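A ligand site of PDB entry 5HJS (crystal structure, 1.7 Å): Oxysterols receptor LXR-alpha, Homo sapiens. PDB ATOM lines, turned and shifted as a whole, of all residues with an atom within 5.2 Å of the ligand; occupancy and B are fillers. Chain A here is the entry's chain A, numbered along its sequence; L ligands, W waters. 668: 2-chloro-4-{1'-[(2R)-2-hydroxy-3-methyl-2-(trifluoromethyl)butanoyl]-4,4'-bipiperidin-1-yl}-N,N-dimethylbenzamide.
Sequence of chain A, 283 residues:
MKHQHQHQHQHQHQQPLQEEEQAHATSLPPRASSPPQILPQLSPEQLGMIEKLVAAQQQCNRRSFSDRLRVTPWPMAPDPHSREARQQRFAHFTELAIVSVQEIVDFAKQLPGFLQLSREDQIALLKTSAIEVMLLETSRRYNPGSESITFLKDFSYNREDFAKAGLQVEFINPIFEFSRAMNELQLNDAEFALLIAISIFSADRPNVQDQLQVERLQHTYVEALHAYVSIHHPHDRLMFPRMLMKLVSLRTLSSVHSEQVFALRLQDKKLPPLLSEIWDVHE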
ATOM      1  N   PHE A  90       3.173  13.823 -10.351  1.00  0.00           N
ATOM      2  CA  PHE A  90       2.976  15.030  -9.536  1.00  0.00           C
ATOM      3  C   PHE A  90       4.341  15.476  -9.003  1.00  0.00           C
ATOM      4  O   PHE A  90       4.668  16.663  -9.098  1.00  0.00           O
ATOM      5  CB  PHE A  90       1.997  14.765  -8.383  1.00  0.00           C
ATOM      6  CG  PHE A  90       1.780  15.941  -7.458  1.00  0.00           C
ATOM      7  CD1 PHE A  90       0.809  16.898  -7.742  1.00  0.00           C
ATOM      8  CD2 PHE A  90       2.537  16.086  -6.308  1.00  0.00           C
ATOM      9  CE1 PHE A  90       0.606  17.977  -6.878  1.00  0.00           C
ATOM     10  CE2 PHE A  90       2.332  17.175  -5.449  1.00  0.00           C
ATOM     11  CZ  PHE A  90       1.371  18.109  -5.736  1.00  0.00           C
ATOM     12  N   PHE A  93       6.655  17.093 -11.757  1.00  0.00           N
ATOM     13  CA  PHE A  93       6.256  18.499 -12.019  1.00  0.00           C
ATOM     14  C   PHE A  93       6.691  19.462 -10.919  1.00  0.00           C
ATOM     15  O   PHE A  93       7.161  20.555 -11.237  1.00  0.00           O
ATOM     16  CB  PHE A  93       4.750  18.595 -12.310  1.00  0.00           C
ATOM     17  CG  PHE A  93       4.384  18.536 -13.786  1.00  0.00           C
ATOM     18  CD1 PHE A  93       4.885  17.520 -14.599  1.00  0.00           C
ATOM     19  CD2 PHE A  93       3.527  19.466 -14.346  1.00  0.00           C
ATOM     20  CE1 PHE A  93       4.545  17.467 -15.962  1.00  0.00           C
ATOM     21  CE2 PHE A  93       3.200  19.419 -15.706  1.00  0.00           C
ATOM     22  CZ  PHE A  93       3.696  18.407 -16.506  1.00  0.00           C
ATOM     23  N   THR A  94       6.557  19.067  -9.629  1.00  0.00           N
ATOM     24  CA  THR A  94       6.978  19.858  -8.475  1.00  0.00           C
ATOM     25  C   THR A  94       8.494  20.070  -8.494  1.00  0.00           C
ATOM     26  O   THR A  94       8.974  21.146  -8.115  1.00  0.00           O
ATOM     27  CB  THR A  94       6.538  19.243  -7.129  1.00  0.00           C
ATOM     28  OG1 THR A  94       7.121  17.955  -6.988  1.00  0.00           O
ATOM     29  CG2 THR A  94       5.044  19.183  -6.935  1.00  0.00           C
ATOM     30  N   LEU A  96      10.416  19.996 -11.312  1.00  0.00           N
ATOM     31  CA  LEU A  96      10.751  20.886 -12.443  1.00  0.00           C
ATOM     32  C   LEU A  96      10.517  22.352 -12.010  1.00  0.00           C
ATOM     33  O   LEU A  96      11.298  23.237 -12.367  1.00  0.00           O
ATOM     34  CB  LEU A  96       9.898  20.571 -13.693  1.00  0.00           C
ATOM     35  CG  LEU A  96      10.113  19.218 -14.371  1.00  0.00           C
ATOM     36  CD1 LEU A  96       9.145  19.029 -15.513  1.00  0.00           C
ATOM     37  CD2 LEU A  96      11.536  19.056 -14.853  1.00  0.00           C
ATOM     38  N   ALA A  97       9.439  22.583 -11.218  1.00  0.00           N
ATOM     39  CA  ALA A  97       9.060  23.900 -10.678  1.00  0.00           C
ATOM     40  C   ALA A  97      10.123  24.446  -9.753  1.00  0.00           C
ATOM     41  O   ALA A  97      10.420  25.639  -9.797  1.00  0.00           O
ATOM     42  CB  ALA A  97       7.748  23.800  -9.954  1.00  0.00           C
ATOM     43  N   VAL A  99      13.391  23.611  -9.811  1.00  0.00           N
ATOM     44  CA  VAL A  99      14.549  23.947 -10.648  1.00  0.00           C
ATOM     45  C   VAL A  99      14.314  25.339 -11.260  1.00  0.00           C
ATOM     46  O   VAL A  99      15.210  26.161 -11.299  1.00  0.00           O
ATOM     47  CB  VAL A  99      14.788  22.854 -11.742  1.00  0.00           C
ATOM     48  CG1 VAL A  99      15.817  23.296 -12.775  1.00  0.00           C
ATOM     49  CG2 VAL A  99      15.197  21.527 -11.120  1.00  0.00           C
ATOM     50  N   SER A 100      13.078  25.587 -11.700  1.00  0.00           N
ATOM     51  CA  SER A 100      12.678  26.853 -12.287  1.00  0.00           C
ATOM     52  C   SER A 100      12.827  27.981 -11.249  1.00  0.00           C
ATOM     53  O   SER A 100      13.468  28.982 -11.570  1.00  0.00           O
ATOM     54  CB  SER A 100      11.248  26.767 -12.825  1.00  0.00           C
ATOM     55  OG  SER A 100      10.986  27.897 -13.644  1.00  0.00           O
ATOM     56  N   GLU A 103      16.463  28.911 -10.758  1.00  0.00           N
ATOM     57  CA  GLU A 103      17.010  29.683 -11.898  1.00  0.00           C
ATOM     58  C   GLU A 103      16.518  31.130 -11.864  1.00  0.00           C
ATOM     59  O   GLU A 103      17.292  32.015 -12.193  1.00  0.00           O
ATOM     60  CB  GLU A 103      16.607  29.028 -13.228  1.00  0.00           C
ATOM     61  CG  GLU A 103      17.345  27.728 -13.498  1.00  0.00           C
ATOM     62  CD  GLU A 103      17.540  27.343 -14.951  1.00  0.00           C
ATOM     63  OE1 GLU A 103      17.255  28.165 -15.844  1.00  0.00           O
ATOM     64  OE2 GLU A 103      17.972  26.189 -15.195  1.00  0.00           O
ATOM     65  N   ILE A 131       5.667  32.632 -10.151  1.00  0.00           N
ATOM     66  CA  ILE A 131       4.723  31.937 -11.029  1.00  0.00           C
ATOM     67  C   ILE A 131       4.607  32.604 -12.417  1.00  0.00           C
ATOM     68  O   ILE A 131       4.494  31.896 -13.396  1.00  0.00           O
ATOM     69  CB  ILE A 131       3.329  31.729 -10.334  1.00  0.00           C
ATOM     70  CG1 ILE A 131       2.418  30.781 -11.157  1.00  0.00           C
ATOM     71  CG2 ILE A 131       2.639  33.043  -9.994  1.00  0.00           C
ATOM     72  CD1 ILE A 131       3.063  29.400 -11.560  1.00  0.00           C
ATOM     73  N   MET A 134       7.798  31.800 -14.279  1.00  0.00           N
ATOM     74  CA  MET A 134       7.731  30.365 -14.639  1.00  0.00           C
ATOM     75  C   MET A 134       6.833  30.144 -15.862  1.00  0.00           C
ATOM     76  O   MET A 134       7.173  29.352 -16.736  1.00  0.00           O
ATOM     77  CB  MET A 134       7.132  29.560 -13.491  1.00  0.00           C
ATOM     78  CG  MET A 134       8.123  29.221 -12.448  1.00  0.00           C
ATOM     79  SD  MET A 134       7.387  28.722 -10.867  1.00  0.00           S
ATOM     80  CE  MET A 134       7.143  27.156 -11.180  1.00  0.00           C
ATOM     81  N   LEU A 135       5.674  30.852 -15.912  1.00  0.00           N
ATOM     82  CA  LEU A 135       4.740  30.719 -17.030  1.00  0.00           C
ATOM     83  C   LEU A 135       5.294  31.388 -18.288  1.00  0.00           C
ATOM     84  O   LEU A 135       4.956  30.939 -19.382  1.00  0.00           O
ATOM     85  CB  LEU A 135       3.318  31.181 -16.665  1.00  0.00           C
ATOM     86  CG  LEU A 135       2.660  30.358 -15.565  1.00  0.00           C
ATOM     87  CD1 LEU A 135       1.389  30.981 -15.124  1.00  0.00           C
ATOM     88  CD2 LEU A 135       2.460  28.867 -15.963  1.00  0.00           C
ATOM     89  N   GLU A 137       8.618  31.368 -18.984  1.00  0.00           N
ATOM     90  CA  GLU A 137       9.617  30.360 -19.372  1.00  0.00           C
ATOM     91  C   GLU A 137       8.898  29.190 -20.033  1.00  0.00           C
ATOM     92  O   GLU A 137       9.415  28.599 -20.973  1.00  0.00           O
ATOM     93  CB  GLU A 137      10.429  29.857 -18.141  1.00  0.00           C
ATOM     94  CG  GLU A 137      11.459  30.821 -17.561  1.00  0.00           C
ATOM     95  CD  GLU A 137      12.639  31.233 -18.419  1.00  0.00           C
ATOM     96  OE1 GLU A 137      12.900  30.578 -19.458  1.00  0.00           O
ATOM     97  OE2 GLU A 137      13.321  32.213 -18.045  1.00  0.00           O
ATOM     98  N   THR A 138       7.686  28.833 -19.532  1.00  0.00           N
ATOM     99  CA  THR A 138       6.856  27.771 -20.100  1.00  0.00           C
ATOM    100  C   THR A 138       6.463  28.155 -21.551  1.00  0.00           C
ATOM    101  O   THR A 138       6.645  27.342 -22.446  1.00  0.00           O
ATOM    102  CB  THR A 138       5.633  27.498 -19.193  1.00  0.00           C
ATOM    103  OG1 THR A 138       6.074  27.055 -17.911  1.00  0.00           O
ATOM    104  CG2 THR A 138       4.708  26.463 -19.769  1.00  0.00           C
ATOM    105  N   ARG A 141       9.039  27.815 -24.212  1.00  0.00           N
ATOM    106  CA  ARG A 141       9.362  26.425 -24.519  1.00  0.00           C
ATOM    107  C   ARG A 141       8.223  25.675 -25.234  1.00  0.00           C
ATOM    108  O   ARG A 141       8.331  24.465 -25.428  1.00  0.00           O
ATOM    109  CB  ARG A 141       9.784  25.721 -23.216  1.00  0.00           C
ATOM    110  CG  ARG A 141      11.171  26.152 -22.749  1.00  0.00           C
ATOM    111  CD  ARG A 141      11.499  25.682 -21.339  1.00  0.00           C
ATOM    112  NE  ARG A 141      12.892  26.009 -20.991  1.00  0.00           N
ATOM    113  CZ  ARG A 141      13.294  27.204 -20.584  1.00  0.00           C
ATOM    114  NH1 ARG A 141      12.425  28.197 -20.462  1.00  0.00           N
ATOM    115  NH2 ARG A 141      14.566  27.421 -20.295  1.00  0.00           N
ATOM    116  N   THR A 150       8.372  21.687 -23.880  1.00  0.00           N
ATOM    117  CA  THR A 150       9.606  20.953 -23.671  1.00  0.00           C
ATOM    118  C   THR A 150      10.380  21.540 -22.477  1.00  0.00           C
ATOM    119  O   THR A 150      10.903  22.646 -22.570  1.00  0.00           O
ATOM    120  CB  THR A 150      10.417  20.931 -24.978  1.00  0.00           C
ATOM    121  OG1 THR A 150       9.643  20.241 -25.962  1.00  0.00           O
ATOM    122  CG2 THR A 150      11.793  20.281 -24.819  1.00  0.00           C
ATOM    123  N   PHE A 151      10.439  20.787 -21.368  1.00  0.00           N
ATOM    124  CA  PHE A 151      11.159  21.184 -20.153  1.00  0.00           C
ATOM    125  C   PHE A 151      12.534  20.527 -20.145  1.00  0.00           C
ATOM    126  O   PHE A 151      12.648  19.343 -20.477  1.00  0.00           O
ATOM    127  CB  PHE A 151      10.380  20.780 -18.885  1.00  0.00           C
ATOM    128  CG  PHE A 151       9.031  21.428 -18.718  1.00  0.00           C
ATOM    129  CD1 PHE A 151       8.921  22.814 -18.585  1.00  0.00           C
ATOM    130  CD2 PHE A 151       7.875  20.672 -18.677  1.00  0.00           C
ATOM    131  CE1 PHE A 151       7.679  23.417 -18.431  1.00  0.00           C
ATOM    132  CE2 PHE A 151       6.624  21.274 -18.519  1.00  0.00           C
ATOM    133  CZ  PHE A 151       6.533  22.638 -18.394  1.00  0.00           C
ATOM    134  N   LEU A 152      13.578  21.294 -19.758  1.00  0.00           N
ATOM    135  CA  LEU A 152      14.976  20.840 -19.658  1.00  0.00           C
ATOM    136  C   LEU A 152      15.508  20.118 -20.913  1.00  0.00           C
ATOM    137  O   LEU A 152      16.081  19.031 -20.806  1.00  0.00           O
ATOM    138  CB  LEU A 152      15.198  19.978 -18.395  1.00  0.00           C
ATOM    139  CG  LEU A 152      15.132  20.678 -17.031  1.00  0.00           C
ATOM    140  CD1 LEU A 152      15.242  19.676 -15.917  1.00  0.00           C
ATOM    141  CD2 LEU A 152      16.194  21.762 -16.897  1.00  0.00           C
ATOM    142  N   LYS A 153      15.317  20.724 -22.105  1.00  0.00           N
ATOM    143  CA  LYS A 153      15.765  20.234 -23.427  1.00  0.00           C
ATOM    144  C   LYS A 153      15.439  18.750 -23.764  1.00  0.00           C
ATOM    145  O   LYS A 153      16.067  18.187 -24.664  1.00  0.00           O
ATOM    146  CB  LYS A 153      17.282  20.502 -23.613  1.00  0.00           C
ATOM    147  CG  LYS A 153      17.624  21.932 -23.991  1.00  0.00           C
ATOM    148  CD  LYS A 153      17.694  22.134 -25.513  1.00  0.00           C
ATOM    149  CE  LYS A 153      16.860  23.303 -25.980  1.00  0.00           C
ATOM    150  NZ  LYS A 153      17.495  24.611 -25.664  1.00  0.00           N
ATOM    151  N   ALA A 165      -0.418  14.816 -14.211  1.00  0.00           N
ATOM    152  CA  ALA A 165       0.473  15.330 -13.161  1.00  0.00           C
ATOM    153  C   ALA A 165      -0.256  16.017 -11.978  1.00  0.00           C
ATOM    154  O   ALA A 165       0.409  16.603 -11.117  1.00  0.00           O
ATOM    155  CB  ALA A 165       1.524  16.253 -13.777  1.00  0.00           C
ATOM    156  N   GLY A 166      -1.590  15.929 -11.952  1.00  0.00           N
ATOM    157  CA  GLY A 166      -2.421  16.473 -10.882  1.00  0.00           C
ATOM    158  C   GLY A 166      -3.014  17.866 -11.060  1.00  0.00           C
ATOM    159  O   GLY A 166      -3.680  18.378 -10.146  1.00  0.00           O
ATOM    160  N   LEU A 167      -2.777  18.499 -12.233  1.00  0.00           N
ATOM    161  CA  LEU A 167      -3.280  19.840 -12.542  1.00  0.00           C
ATOM    162  C   LEU A 167      -4.732  19.803 -12.970  1.00  0.00           C
ATOM    163  O   LEU A 167      -5.137  18.886 -13.673  1.00  0.00           O
ATOM    164  CB  LEU A 167      -2.436  20.510 -13.639  1.00  0.00           C
ATOM    165  CG  LEU A 167      -1.121  21.142 -13.214  1.00  0.00           C
ATOM    166  CD1 LEU A 167       0.032  20.173 -13.356  1.00  0.00           C
ATOM    167  CD2 LEU A 167      -0.824  22.389 -14.023  1.00  0.00           C
ATOM    168  N   PHE A 171      -6.737  25.362 -14.974  1.00  0.00           N
ATOM    169  CA  PHE A 171      -5.401  25.958 -14.978  1.00  0.00           C
ATOM    170  C   PHE A 171      -4.613  25.561 -16.213  1.00  0.00           C
ATOM    171  O   PHE A 171      -3.891  26.386 -16.748  1.00  0.00           O
ATOM    172  CB  PHE A 171      -4.599  25.604 -13.697  1.00  0.00           C
ATOM    173  CG  PHE A 171      -3.234  26.231 -13.541  1.00  0.00           C
ATOM    174  CD1 PHE A 171      -3.008  27.575 -13.842  1.00  0.00           C
ATOM    175  CD2 PHE A 171      -2.174  25.499 -13.020  1.00  0.00           C
ATOM    176  CE1 PHE A 171      -1.745  28.147 -13.689  1.00  0.00           C
ATOM    177  CE2 PHE A 171      -0.915  26.078 -12.831  1.00  0.00           C
ATOM    178  CZ  PHE A 171      -0.700  27.397 -13.175  1.00  0.00           C
ATOM    179  N   HIS A 257      -3.595  30.298 -10.865  1.00  0.00           N
ATOM    180  CA  HIS A 257      -2.661  29.404 -10.160  1.00  0.00           C
ATOM    181  C   HIS A 257      -2.972  29.388  -8.659  1.00  0.00           C
ATOM    182  O   HIS A 257      -2.910  28.330  -8.043  1.00  0.00           O
ATOM    183  CB  HIS A 257      -1.199  29.778 -10.425  1.00  0.00           C
ATOM    184  CG  HIS A 257      -0.233  29.060  -9.526  1.00  0.00           C
ATOM    185  ND1 HIS A 257       0.367  29.692  -8.466  1.00  0.00           N
ATOM    186  CD2 HIS A 257       0.181  27.767  -9.553  1.00  0.00           C
ATOM    187  CE1 HIS A 257       1.155  28.799  -7.907  1.00  0.00           C
ATOM    188  NE2 HIS A 257       1.073  27.625  -8.521  1.00  0.00           N
ATOM    189  N   GLN A 260      -5.607  26.968  -8.041  1.00  0.00           N
ATOM    190  CA  GLN A 260      -5.032  25.648  -8.213  1.00  0.00           C
ATOM    191  C   GLN A 260      -4.325  25.202  -6.900  1.00  0.00           C
ATOM    192  O   GLN A 260      -4.449  24.037  -6.507  1.00  0.00           O
ATOM    193  CB  GLN A 260      -4.043  25.643  -9.377  1.00  0.00           C
ATOM    194  CG  GLN A 260      -3.162  24.385  -9.463  1.00  0.00           C
ATOM    195  CD  GLN A 260      -3.927  23.131  -9.850  1.00  0.00           C
ATOM    196  OE1 GLN A 260      -4.048  22.809 -11.023  1.00  0.00           O
ATOM    197  NE2 GLN A 260      -4.458  22.411  -8.870  1.00  0.00           N
ATOM    198  N   VAL A 261      -3.585  26.131  -6.249  1.00  0.00           N
ATOM    199  CA  VAL A 261      -2.861  25.876  -5.004  1.00  0.00           C
ATOM    200  C   VAL A 261      -3.887  25.562  -3.899  1.00  0.00           C
ATOM    201  O   VAL A 261      -3.672  24.620  -3.139  1.00  0.00           O
ATOM    202  CB  VAL A 261      -1.873  27.038  -4.647  1.00  0.00           C
ATOM    203  CG1 VAL A 261      -1.413  26.988  -3.189  1.00  0.00           C
ATOM    204  CG2 VAL A 261      -0.668  27.017  -5.576  1.00  0.00           C
ATOM    205  N   LEU A 264      -5.287  22.051  -4.311  1.00  0.00           N
ATOM    206  CA  LEU A 264      -4.345  21.026  -3.850  1.00  0.00           C
ATOM    207  C   LEU A 264      -4.425  20.822  -2.348  1.00  0.00           C
ATOM    208  O   LEU A 264      -4.228  19.690  -1.885  1.00  0.00           O
ATOM    209  CB  LEU A 264      -2.888  21.293  -4.277  1.00  0.00           C
ATOM    210  CG  LEU A 264      -2.565  21.266  -5.756  1.00  0.00           C
ATOM    211  CD1 LEU A 264      -1.151  21.786  -6.000  1.00  0.00           C
ATOM    212  CD2 LEU A 264      -2.707  19.872  -6.339  1.00  0.00           C
ATOM    213  N   LEU A 271       2.673  20.278  -1.251  1.00  0.00           N
ATOM    214  CA  LEU A 271       3.716  20.814  -2.105  1.00  0.00           C
ATOM    215  C   LEU A 271       5.053  20.663  -1.365  1.00  0.00           C
ATOM    216  O   LEU A 271       5.056  20.697  -0.126  1.00  0.00           O
ATOM    217  CB  LEU A 271       3.430  22.302  -2.428  1.00  0.00           C
ATOM    218  CG  LEU A 271       2.357  22.592  -3.475  1.00  0.00           C
ATOM    219  CD1 LEU A 271       2.027  24.057  -3.499  1.00  0.00           C
ATOM    220  CD2 LEU A 271       2.798  22.153  -4.852  1.00  0.00           C
ATOM    221  N   LEU A 275       8.142  25.285  -2.662  1.00  0.00           N
ATOM    222  CA  LEU A 275       6.902  25.699  -3.298  1.00  0.00           C
ATOM    223  C   LEU A 275       5.859  26.013  -2.267  1.00  0.00           C
ATOM    224  O   LEU A 275       5.109  26.975  -2.435  1.00  0.00           O
ATOM    225  CB  LEU A 275       6.397  24.651  -4.319  1.00  0.00           C
ATOM    226  CG  LEU A 275       7.364  24.241  -5.430  1.00  0.00           C
ATOM    227  CD1 LEU A 275       6.719  23.263  -6.372  1.00  0.00           C
ATOM    228  CD2 LEU A 275       7.957  25.467  -6.173  1.00  0.00           C
ATOM    229  N   TRP A 279       4.144  29.697  -2.123  1.00  0.00           N
ATOM    230  CA  TRP A 279       2.742  29.666  -2.543  1.00  0.00           C
ATOM    231  C   TRP A 279       1.668  29.387  -1.527  1.00  0.00           C
ATOM    232  O   TRP A 279       0.567  29.886  -1.705  1.00  0.00           O
ATOM    233  CB  TRP A 279       2.569  28.676  -3.684  1.00  0.00           C
ATOM    234  CG  TRP A 279       3.305  29.056  -4.928  1.00  0.00           C
ATOM    235  CD1 TRP A 279       3.631  30.314  -5.342  1.00  0.00           C
ATOM    236  CD2 TRP A 279       3.790  28.156  -5.937  1.00  0.00           C
ATOM    237  NE1 TRP A 279       4.282  30.263  -6.547  1.00  0.00           N
ATOM    238  CE2 TRP A 279       4.382  28.958  -6.950  1.00  0.00           C
ATOM    239  CE3 TRP A 279       3.692  26.767  -6.143  1.00  0.00           C
ATOM    240  CZ2 TRP A 279       4.928  28.403  -8.112  1.00  0.00           C
ATOM    241  CZ3 TRP A 279       4.239  26.226  -7.301  1.00  0.00           C
ATOM    242  CH2 TRP A 279       4.856  27.036  -8.266  1.00  0.00           C
HETATM  243  F2  668 L   1       0.277  21.102  -8.997  1.00  0.00           F
HETATM  244  C24 668 L   1       0.514  22.273  -9.582  1.00  0.00           C
HETATM  245  F   668 L   1      -0.351  23.148  -9.074  1.00  0.00           F
HETATM  246  F1  668 L   1       0.195  22.139 -10.865  1.00  0.00           F
HETATM  247  C3  668 L   1       1.961  22.737  -9.403  1.00  0.00           C
HETATM  248  O   668 L   1       2.107  22.919  -7.996  1.00  0.00           O
HETATM  249  C1  668 L   1       3.078  21.771  -9.867  1.00  0.00           C
HETATM  250  C2  668 L   1       2.854  20.341  -9.394  1.00  0.00           C
HETATM  251  C   668 L   1       4.466  22.253  -9.460  1.00  0.00           C
HETATM  252  C4  668 L   1       2.044  24.097 -10.122  1.00  0.00           C
HETATM  253  O1  668 L   1       1.769  25.016  -9.377  1.00  0.00           O
HETATM  254  N   668 L   1       2.297  24.321 -11.428  1.00  0.00           N
HETATM  255  C9  668 L   1       2.619  25.681 -11.867  1.00  0.00           C
HETATM  256  C8  668 L   1       4.055  25.771 -12.338  1.00  0.00           C
HETATM  257  C7  668 L   1       4.368  24.752 -13.441  1.00  0.00           C
HETATM  258  C6  668 L   1       3.886  23.348 -13.046  1.00  0.00           C
HETATM  259  C5  668 L   1       2.446  23.393 -12.557  1.00  0.00           C
HETATM  260  C10 668 L   1       5.834  24.761 -13.836  1.00  0.00           C
HETATM  261  C14 668 L   1       6.291  23.484 -14.547  1.00  0.00           C
HETATM  262  C13 668 L   1       7.801  23.518 -14.733  1.00  0.00           C
HETATM  263  N1  668 L   1       8.165  24.803 -15.458  1.00  0.00           N
HETATM  264  C12 668 L   1       7.760  26.057 -14.733  1.00  0.00           C
HETATM  265  C11 668 L   1       6.241  25.991 -14.652  1.00  0.00           C
HETATM  266  C15 668 L   1       9.550  24.921 -15.959  1.00  0.00           C
HETATM  267  C23 668 L   1      10.482  23.991 -15.556  1.00  0.00           C
HETATM  268  C22 668 L   1      11.742  24.016 -16.126  1.00  0.00           C
HETATM  269 CL   668 L   1      12.905  22.879 -15.552  1.00  0.00          CL
HETATM  270  C18 668 L   1      12.079  24.948 -17.103  1.00  0.00           C
HETATM  271  C17 668 L   1      11.117  25.896 -17.477  1.00  0.00           C
HETATM  272  C16 668 L   1       9.857  25.894 -16.908  1.00  0.00           C
HETATM  273  C19 668 L   1      13.424  24.926 -17.792  1.00  0.00           C
HETATM  274  O2  668 L   1      13.546  24.249 -18.795  1.00  0.00           O
HETATM  275  N2  668 L   1      14.431  25.614 -17.242  1.00  0.00           N
HETATM  276  C21 668 L   1      15.794  25.563 -17.791  1.00  0.00           C
HETATM  277  C20 668 L   1      14.302  26.425 -16.035  1.00  0.00           C
HETATM  278  O   HOH W   1      13.093  29.307 -14.645  1.00  0.00           O
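NE2 of His 257 lies within hydrogen-bond range of O1 of the ligand (2.8 Å).
NE of Arg 141 is in hydrogen-bond range of O2 of the ligand (2.9 Å).
The backbone NH (N) of Leu 152 is in hydrogen-bond range of an oxygen (O2) of the ligand (3.1 Å).
The guanidinium group of Arg 141 lies within salt-bridge range of the side-chain carboxylate of Glu 137 (2.6 Å).
The backbone NH (N) of Thr 150 sits at hydrogen-bond distance from the backbone carbonyl oxygen (O) of Arg 141, at 3.2 Å.
The backbone carbonyl oxygen (O) of Met 134 sits at hydrogen-bond distance from the side-chain hydroxyl (OG1) of Thr 138 (2.8 Å).
The backbone carbonyl oxygen (O) of Phe 90 sits close to the side-chain hydroxyl (OG1) of Thr 94, at 3.5 Å.
Phe 90 touches the ligand.
Phe 93 touches the ligand (O to C, 3.6 Å).
Thr 94 touches the ligand.
O of Leu 96 touches C23 of the ligand, at 3.4 Å.
Ala 97 touches the ligand.
OG of Ser 100 touches C12 of the ligand, 3.9 Å away.
Glu 103 touches the ligand (OE1 to C20, 3.4 Å).
Ile 131 touches the ligand.
CE of Met 134 touches C8 of the ligand (3.6 Å).
Thr 138 touches the ligand (OG1 to C11, 3.4 Å).
Phe 151 touches the ligand.
Leu 167 touches the ligand (CG to F1, 2.9 Å).
Phe 171 touches the ligand.
Gln 260 touches the ligand.
Leu 264 touches the ligand.
Leu 271 touches the ligand.
CD1 of Leu 275 touches C of the ligand, 3.95 Å away.
Trp 279 touches the ligand (CZ3 to O1, 3.4 Å).
21 residues have an atom within 4 Å of the ligand: Phe 90, Phe 93, Thr 94, Leu 96, Ala 97, Ser 100, Glu 103, Ile 131, Met 134, Thr 138, Arg 141, Phe 151, Leu 152, Leu 167, Phe 171, His 257, Gln 260, Leu 264, Leu 271, Leu 275 and Trp 279.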
